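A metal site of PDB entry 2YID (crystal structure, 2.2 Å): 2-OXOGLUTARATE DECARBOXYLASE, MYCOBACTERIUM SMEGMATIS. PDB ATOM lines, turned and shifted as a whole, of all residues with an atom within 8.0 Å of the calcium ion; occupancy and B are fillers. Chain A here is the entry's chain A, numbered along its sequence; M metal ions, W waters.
The side-chain carboxylate of Asp 645 sits close to the backbone NH of Arg 703.
Within 4 Å of the calcium ion: Asp 645, His 696, Asp 699 and Ile 701.
The nearest printed residue that does not touch the calcium ion is Gln 702 (4.5 Å).
The calcium ion is bound by the backbone carbonyl oxygen (O) of Ile 701 (2.3 Å), the backbone carbonyl oxygen (O) of His 696 (2.4 Å), water W1 (2.4 Å), the side-chain carboxylate (OD1) of Asp 699 (2.4 Å), the side-chain carboxylate (OD2) of Asp 645 (2.5 Å), the side-chain carboxylate (OD1) of Asp 645 (2.5 Å) and water W2 (2.6 Å).
The calcium ion has seven donor atoms within binding distance.
Water W2 lies within hydrogen-bond range of OD2 of Asp 699 (2.9 Å), ND1 of His 696 (2.9 Å) and O of Arg 703 (3.4 Å).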
ATOM      1  N   GLN A 466       4.588 -15.112  -9.942  1.00  0.00           N
ATOM      2  CA  GLN A 466       4.604 -16.009 -11.095  1.00  0.00           C
ATOM      3  C   GLN A 466       3.214 -16.015 -11.773  1.00  0.00           C
ATOM      4  O   GLN A 466       2.243 -16.526 -11.196  1.00  0.00           O
ATOM      5  CB  GLN A 466       5.021 -17.414 -10.689  1.00  0.00           C
ATOM      6  CG  GLN A 466       6.431 -17.516 -10.153  1.00  0.00           C
ATOM      7  CD  GLN A 466       6.747 -18.973  -9.952  1.00  0.00           C
ATOM      8  OE1 GLN A 466       7.114 -19.663 -10.896  1.00  0.00           O
ATOM      9  NE2 GLN A 466       6.540 -19.480  -8.726  1.00  0.00           N
ATOM     10  N   LYS A 535      11.532 -33.099 -22.498  1.00  0.00           N
ATOM     11  CA  LYS A 535      11.481 -32.933 -21.042  1.00  0.00           C
ATOM     12  C   LYS A 535      11.927 -34.161 -20.263  1.00  0.00           C
ATOM     13  O   LYS A 535      11.551 -35.293 -20.594  1.00  0.00           O
ATOM     14  CB  LYS A 535      10.069 -32.549 -20.590  1.00  0.00           C
ATOM     15  CG  LYS A 535      10.065 -31.661 -19.364  1.00  0.00           C
ATOM     16  CD  LYS A 535       8.707 -31.103 -19.092  1.00  0.00           C
ATOM     17  CE  LYS A 535       8.723 -30.333 -17.801  1.00  0.00           C
ATOM     18  NZ  LYS A 535       9.419 -29.040 -17.963  1.00  0.00           N
ATOM     19  N   PRO A 608      14.607 -27.185 -12.223  1.00  0.00           N
ATOM     20  CA  PRO A 608      13.287 -26.569 -12.517  1.00  0.00           C
ATOM     21  C   PRO A 608      12.651 -26.999 -13.851  1.00  0.00           C
ATOM     22  O   PRO A 608      11.427 -26.880 -14.021  1.00  0.00           O
ATOM     23  CB  PRO A 608      13.589 -25.056 -12.533  1.00  0.00           C
ATOM     24  CG  PRO A 608      14.917 -24.911 -11.874  1.00  0.00           C
ATOM     25  CD  PRO A 608      15.668 -26.171 -12.081  1.00  0.00           C
ATOM     26  N   ALA A 610      12.657 -30.087 -14.987  1.00  0.00           N
ATOM     27  CA  ALA A 610      12.192 -31.469 -14.890  1.00  0.00           C
ATOM     28  C   ALA A 610      10.704 -31.519 -14.501  1.00  0.00           C
ATOM     29  O   ALA A 610      10.201 -30.636 -13.822  1.00  0.00           O
ATOM     30  CB  ALA A 610      13.024 -32.238 -13.873  1.00  0.00           C
ATOM     31  N   MET A 611      10.017 -32.588 -14.948  1.00  0.00           N
ATOM     32  CA  MET A 611       8.657 -32.945 -14.580  1.00  0.00           C
ATOM     33  C   MET A 611       8.862 -33.974 -13.463  1.00  0.00           C
ATOM     34  O   MET A 611       9.440 -35.031 -13.717  1.00  0.00           O
ATOM     35  CB  MET A 611       7.870 -33.499 -15.793  1.00  0.00           C
ATOM     36  CG  MET A 611       6.430 -33.893 -15.488  1.00  0.00           C
ATOM     37  SD  MET A 611       5.291 -32.485 -15.395  1.00  0.00           S
ATOM     38  CE  MET A 611       3.811 -33.295 -15.028  1.00  0.00           C
ATOM     39  N   SER A 644       9.524 -24.712  -6.414  1.00  0.00           N
ATOM     40  CA  SER A 644       9.411 -26.140  -6.668  1.00  0.00           C
ATOM     41  C   SER A 644       8.172 -26.391  -7.495  1.00  0.00           C
ATOM     42  O   SER A 644       7.150 -25.784  -7.259  1.00  0.00           O
ATOM     43  CB  SER A 644       9.337 -26.899  -5.351  1.00  0.00           C
ATOM     44  OG  SER A 644       8.983 -28.244  -5.557  1.00  0.00           O
ATOM     45  N   ASP A 645       8.284 -27.288  -8.466  1.00  0.00           N
ATOM     46  CA  ASP A 645       7.207 -27.647  -9.365  1.00  0.00           C
ATOM     47  C   ASP A 645       6.780 -29.103  -9.108  1.00  0.00           C
ATOM     48  O   ASP A 645       6.153 -29.724  -9.976  1.00  0.00           O
ATOM     49  CB  ASP A 645       7.695 -27.458 -10.826  1.00  0.00           C
ATOM     50  CG  ASP A 645       6.641 -27.002 -11.812  1.00  0.00           C
ATOM     51  OD1 ASP A 645       5.703 -26.282 -11.393  1.00  0.00           O
ATOM     52  OD2 ASP A 645       6.795 -27.288 -13.022  1.00  0.00           O
ATOM     53  N   VAL A 646       7.096 -29.646  -7.913  1.00  0.00           N
ATOM     54  CA  VAL A 646       6.799 -31.041  -7.577  1.00  0.00           C
ATOM     55  C   VAL A 646       5.281 -31.369  -7.707  1.00  0.00           C
ATOM     56  O   VAL A 646       4.431 -30.542  -7.385  1.00  0.00           O
ATOM     57  CB  VAL A 646       7.366 -31.460  -6.181  1.00  0.00           C
ATOM     58  CG1 VAL A 646       6.664 -30.749  -5.016  1.00  0.00           C
ATOM     59  CG2 VAL A 646       7.354 -32.975  -6.012  1.00  0.00           C
ATOM     60  N   VAL A 647       4.982 -32.551  -8.262  1.00  0.00           N
ATOM     61  CA  VAL A 647       3.616 -33.045  -8.404  1.00  0.00           C
ATOM     62  C   VAL A 647       3.400 -34.133  -7.360  1.00  0.00           C
ATOM     63  O   VAL A 647       4.164 -35.076  -7.308  1.00  0.00           O
ATOM     64  CB  VAL A 647       3.272 -33.567  -9.820  1.00  0.00           C
ATOM     65  CG1 VAL A 647       1.804 -34.036  -9.901  1.00  0.00           C
ATOM     66  CG2 VAL A 647       3.553 -32.521 -10.891  1.00  0.00           C
ATOM     67  N   THR A 679      -1.296 -25.529  -6.933  1.00  0.00           N
ATOM     68  CA  THR A 679      -2.473 -25.857  -7.707  1.00  0.00           C
ATOM     69  C   THR A 679      -3.007 -27.129  -7.071  1.00  0.00           C
ATOM     70  O   THR A 679      -2.233 -28.034  -6.752  1.00  0.00           O
ATOM     71  CB  THR A 679      -2.174 -25.998  -9.218  1.00  0.00           C
ATOM     72  OG1 THR A 679      -1.551 -24.797  -9.688  1.00  0.00           O
ATOM     73  CG2 THR A 679      -3.444 -26.247 -10.038  1.00  0.00           C
ATOM     74  N   LEU A 692      -3.982 -31.257 -17.561  1.00  0.00           N
ATOM     75  CA  LEU A 692      -3.518 -30.728 -16.278  1.00  0.00           C
ATOM     76  C   LEU A 692      -2.013 -30.974 -16.122  1.00  0.00           C
ATOM     77  O   LEU A 692      -1.284 -30.060 -15.726  1.00  0.00           O
ATOM     78  CB  LEU A 692      -4.300 -31.399 -15.112  1.00  0.00           C
ATOM     79  CG  LEU A 692      -3.881 -30.984 -13.690  1.00  0.00           C
ATOM     80  CD1 LEU A 692      -4.435 -29.607 -13.335  1.00  0.00           C
ATOM     81  CD2 LEU A 692      -4.283 -32.033 -12.669  1.00  0.00           C
ATOM     82  N   LEU A 693      -1.556 -32.204 -16.439  1.00  0.00           N
ATOM     83  CA  LEU A 693      -0.134 -32.557 -16.331  1.00  0.00           C
ATOM     84  C   LEU A 693       0.693 -31.821 -17.383  1.00  0.00           C
ATOM     85  O   LEU A 693       1.790 -31.363 -17.064  1.00  0.00           O
ATOM     86  CB  LEU A 693       0.083 -34.064 -16.446  1.00  0.00           C
ATOM     87  CG  LEU A 693      -0.351 -34.942 -15.275  1.00  0.00           C
ATOM     88  CD1 LEU A 693      -0.153 -36.429 -15.595  1.00  0.00           C
ATOM     89  CD2 LEU A 693       0.388 -34.575 -13.996  1.00  0.00           C
ATOM     90  N   ARG A 694       0.176 -31.692 -18.624  1.00  0.00           N
ATOM     91  CA  ARG A 694       0.905 -30.974 -19.674  1.00  0.00           C
ATOM     92  C   ARG A 694       0.977 -29.479 -19.358  1.00  0.00           C
ATOM     93  O   ARG A 694       2.065 -28.910 -19.500  1.00  0.00           O
ATOM     94  CB  ARG A 694       0.307 -31.243 -21.055  1.00  0.00           C
ATOM     95  CG  ARG A 694       0.743 -32.603 -21.556  1.00  0.00           C
ATOM     96  CD  ARG A 694       0.343 -32.911 -22.960  1.00  0.00           C
ATOM     97  NE  ARG A 694       0.719 -31.882 -23.953  1.00  0.00           N
ATOM     98  CZ  ARG A 694       1.915 -31.750 -24.500  1.00  0.00           C
ATOM     99  NH1 ARG A 694       2.920 -32.542 -24.144  1.00  0.00           N
ATOM    100  NH2 ARG A 694       2.131 -30.803 -25.413  1.00  0.00           N
ATOM    101  N   ARG A 695      -0.126 -28.875 -18.850  1.00  0.00           N
ATOM    102  CA  ARG A 695      -0.147 -27.458 -18.464  1.00  0.00           C
ATOM    103  C   ARG A 695       0.895 -27.239 -17.369  1.00  0.00           C
ATOM    104  O   ARG A 695       1.664 -26.279 -17.437  1.00  0.00           O
ATOM    105  CB  ARG A 695      -1.546 -26.989 -18.015  1.00  0.00           C
ATOM    106  CG  ARG A 695      -1.653 -25.473 -17.741  1.00  0.00           C
ATOM    107  CD  ARG A 695      -3.014 -25.034 -17.201  1.00  0.00           C
ATOM    108  NE  ARG A 695      -3.296 -25.568 -15.857  1.00  0.00           N
ATOM    109  CZ  ARG A 695      -4.248 -25.120 -15.035  1.00  0.00           C
ATOM    110  NH1 ARG A 695      -5.016 -24.095 -15.392  1.00  0.00           N
ATOM    111  NH2 ARG A 695      -4.434 -25.686 -13.845  1.00  0.00           N
ATOM    112  N   HIS A 696       0.981 -28.171 -16.403  1.00  0.00           N
ATOM    113  CA  HIS A 696       1.926 -28.103 -15.312  1.00  0.00           C
ATOM    114  C   HIS A 696       3.385 -28.129 -15.800  1.00  0.00           C
ATOM    115  O   HIS A 696       4.211 -27.377 -15.301  1.00  0.00           O
ATOM    116  CB  HIS A 696       1.697 -29.229 -14.318  1.00  0.00           C
ATOM    117  CG  HIS A 696       2.596 -29.109 -13.122  1.00  0.00           C
ATOM    118  ND1 HIS A 696       2.349 -28.183 -12.136  1.00  0.00           N
ATOM    119  CD2 HIS A 696       3.767 -29.734 -12.862  1.00  0.00           C
ATOM    120  CE1 HIS A 696       3.335 -28.317 -11.271  1.00  0.00           C
ATOM    121  NE2 HIS A 696       4.223 -29.228 -11.671  1.00  0.00           N
ATOM    122  N   GLY A 697       3.705 -29.018 -16.735  1.00  0.00           N
ATOM    123  CA  GLY A 697       5.056 -29.121 -17.250  1.00  0.00           C
ATOM    124  C   GLY A 697       5.466 -28.076 -18.276  1.00  0.00           C
ATOM    125  O   GLY A 697       6.655 -27.863 -18.483  1.00  0.00           O
ATOM    126  N   LYS A 698       4.502 -27.395 -18.911  1.00  0.00           N
ATOM    127  CA  LYS A 698       4.781 -26.444 -19.976  1.00  0.00           C
ATOM    128  C   LYS A 698       4.518 -24.969 -19.639  1.00  0.00           C
ATOM    129  O   LYS A 698       4.882 -24.109 -20.441  1.00  0.00           O
ATOM    130  CB  LYS A 698       3.934 -26.809 -21.216  1.00  0.00           C
ATOM    131  CG  LYS A 698       4.329 -28.144 -21.854  1.00  0.00           C
ATOM    132  CD  LYS A 698       3.359 -28.587 -22.946  1.00  0.00           C
ATOM    133  CE  LYS A 698       3.536 -27.876 -24.261  1.00  0.00           C
ATOM    134  NZ  LYS A 698       4.858 -28.158 -24.879  1.00  0.00           N
ATOM    135  N   ASP A 699       3.882 -24.658 -18.490  1.00  0.00           N
ATOM    136  CA  ASP A 699       3.491 -23.280 -18.138  1.00  0.00           C
ATOM    137  C   ASP A 699       4.655 -22.358 -17.767  1.00  0.00           C
ATOM    138  O   ASP A 699       4.451 -21.165 -17.684  1.00  0.00           O
ATOM    139  CB  ASP A 699       2.471 -23.280 -16.978  1.00  0.00           C
ATOM    140  CG  ASP A 699       2.886 -23.969 -15.664  1.00  0.00           C
ATOM    141  OD1 ASP A 699       4.098 -24.253 -15.485  1.00  0.00           O
ATOM    142  OD2 ASP A 699       1.995 -24.195 -14.815  1.00  0.00           O
ATOM    143  N   GLY A 700       5.818 -22.923 -17.445  1.00  0.00           N
ATOM    144  CA  GLY A 700       6.998 -22.174 -17.008  1.00  0.00           C
ATOM    145  C   GLY A 700       6.917 -21.609 -15.602  1.00  0.00           C
ATOM    146  O   GLY A 700       7.782 -20.805 -15.216  1.00  0.00           O
ATOM    147  N   ILE A 701       5.887 -21.997 -14.832  1.00  0.00           N
ATOM    148  CA  ILE A 701       5.660 -21.592 -13.429  1.00  0.00           C
ATOM    149  C   ILE A 701       6.214 -22.702 -12.582  1.00  0.00           C
ATOM    150  O   ILE A 701       6.040 -23.866 -12.931  1.00  0.00           O
ATOM    151  CB  ILE A 701       4.135 -21.322 -13.168  1.00  0.00           C
ATOM    152  CG1 ILE A 701       3.713 -19.977 -13.748  1.00  0.00           C
ATOM    153  CG2 ILE A 701       3.755 -21.376 -11.694  1.00  0.00           C
ATOM    154  CD1 ILE A 701       2.949 -20.103 -14.951  1.00  0.00           C
ATOM    155  N   GLN A 702       6.932 -22.356 -11.508  1.00  0.00           N
ATOM    156  CA  GLN A 702       7.503 -23.357 -10.627  1.00  0.00           C
ATOM    157  C   GLN A 702       6.682 -23.360  -9.353  1.00  0.00           C
ATOM    158  O   GLN A 702       7.051 -22.698  -8.375  1.00  0.00           O
ATOM    159  CB  GLN A 702       9.005 -23.107 -10.372  1.00  0.00           C
ATOM    160  CG  GLN A 702       9.874 -23.019 -11.627  1.00  0.00           C
ATOM    161  CD  GLN A 702       9.818 -24.309 -12.414  1.00  0.00           C
ATOM    162  OE1 GLN A 702      10.138 -25.384 -11.899  1.00  0.00           O
ATOM    163  NE2 GLN A 702       9.375 -24.230 -13.663  1.00  0.00           N
ATOM    164  N   ARG A 703       5.552 -24.067  -9.386  1.00  0.00           N
ATOM    165  CA  ARG A 703       4.637 -24.168  -8.234  1.00  0.00           C
ATOM    166  C   ARG A 703       4.105 -25.576  -8.137  1.00  0.00           C
ATOM    167  O   ARG A 703       3.764 -26.198  -9.152  1.00  0.00           O
ATOM    168  CB  ARG A 703       3.506 -23.129  -8.285  1.00  0.00           C
ATOM    169  CG  ARG A 703       3.990 -21.804  -7.797  1.00  0.00           C
ATOM    170  CD  ARG A 703       3.022 -20.653  -7.984  1.00  0.00           C
ATOM    171  NE  ARG A 703       3.598 -19.444  -7.387  1.00  0.00           N
ATOM    172  CZ  ARG A 703       3.038 -18.237  -7.431  1.00  0.00           C
ATOM    173  NH1 ARG A 703       1.876 -18.053  -8.037  1.00  0.00           N
ATOM    174  NH2 ARG A 703       3.642 -17.200  -6.855  1.00  0.00           N
ATOM    175  N   PRO A 704       4.063 -26.123  -6.885  1.00  0.00           N
ATOM    176  CA  PRO A 704       3.636 -27.500  -6.720  1.00  0.00           C
ATOM    177  C   PRO A 704       2.203 -27.729  -7.169  1.00  0.00           C
ATOM    178  O   PRO A 704       1.369 -26.813  -7.162  1.00  0.00           O
ATOM    179  CB  PRO A 704       3.801 -27.761  -5.223  1.00  0.00           C
ATOM    180  CG  PRO A 704       4.751 -26.737  -4.762  1.00  0.00           C
ATOM    181  CD  PRO A 704       4.448 -25.529  -5.591  1.00  0.00           C
ATOM    182  N   LEU A 705       1.941 -28.962  -7.625  1.00  0.00           N
ATOM    183  CA  LEU A 705       0.628 -29.375  -8.070  1.00  0.00           C
ATOM    184  C   LEU A 705       0.203 -30.575  -7.225  1.00  0.00           C
ATOM    185  O   LEU A 705       0.913 -31.568  -7.155  1.00  0.00           O
ATOM    186  CB  LEU A 705       0.625 -29.695  -9.583  1.00  0.00           C
ATOM    187  CG  LEU A 705      -0.530 -30.515 -10.155  1.00  0.00           C
ATOM    188  CD1 LEU A 705      -1.883 -29.776 -10.047  1.00  0.00           C
ATOM    189  CD2 LEU A 705      -0.259 -30.890 -11.580  1.00  0.00           C
HETATM  190 CA    CA M   1       5.030 -25.743 -13.780  1.00  0.00          CA
HETATM  191  O   HOH W   1       6.885 -25.519 -15.291  1.00  0.00           O
HETATM  192  O   HOH W   2       2.890 -25.320 -12.347  1.00  0.00           O
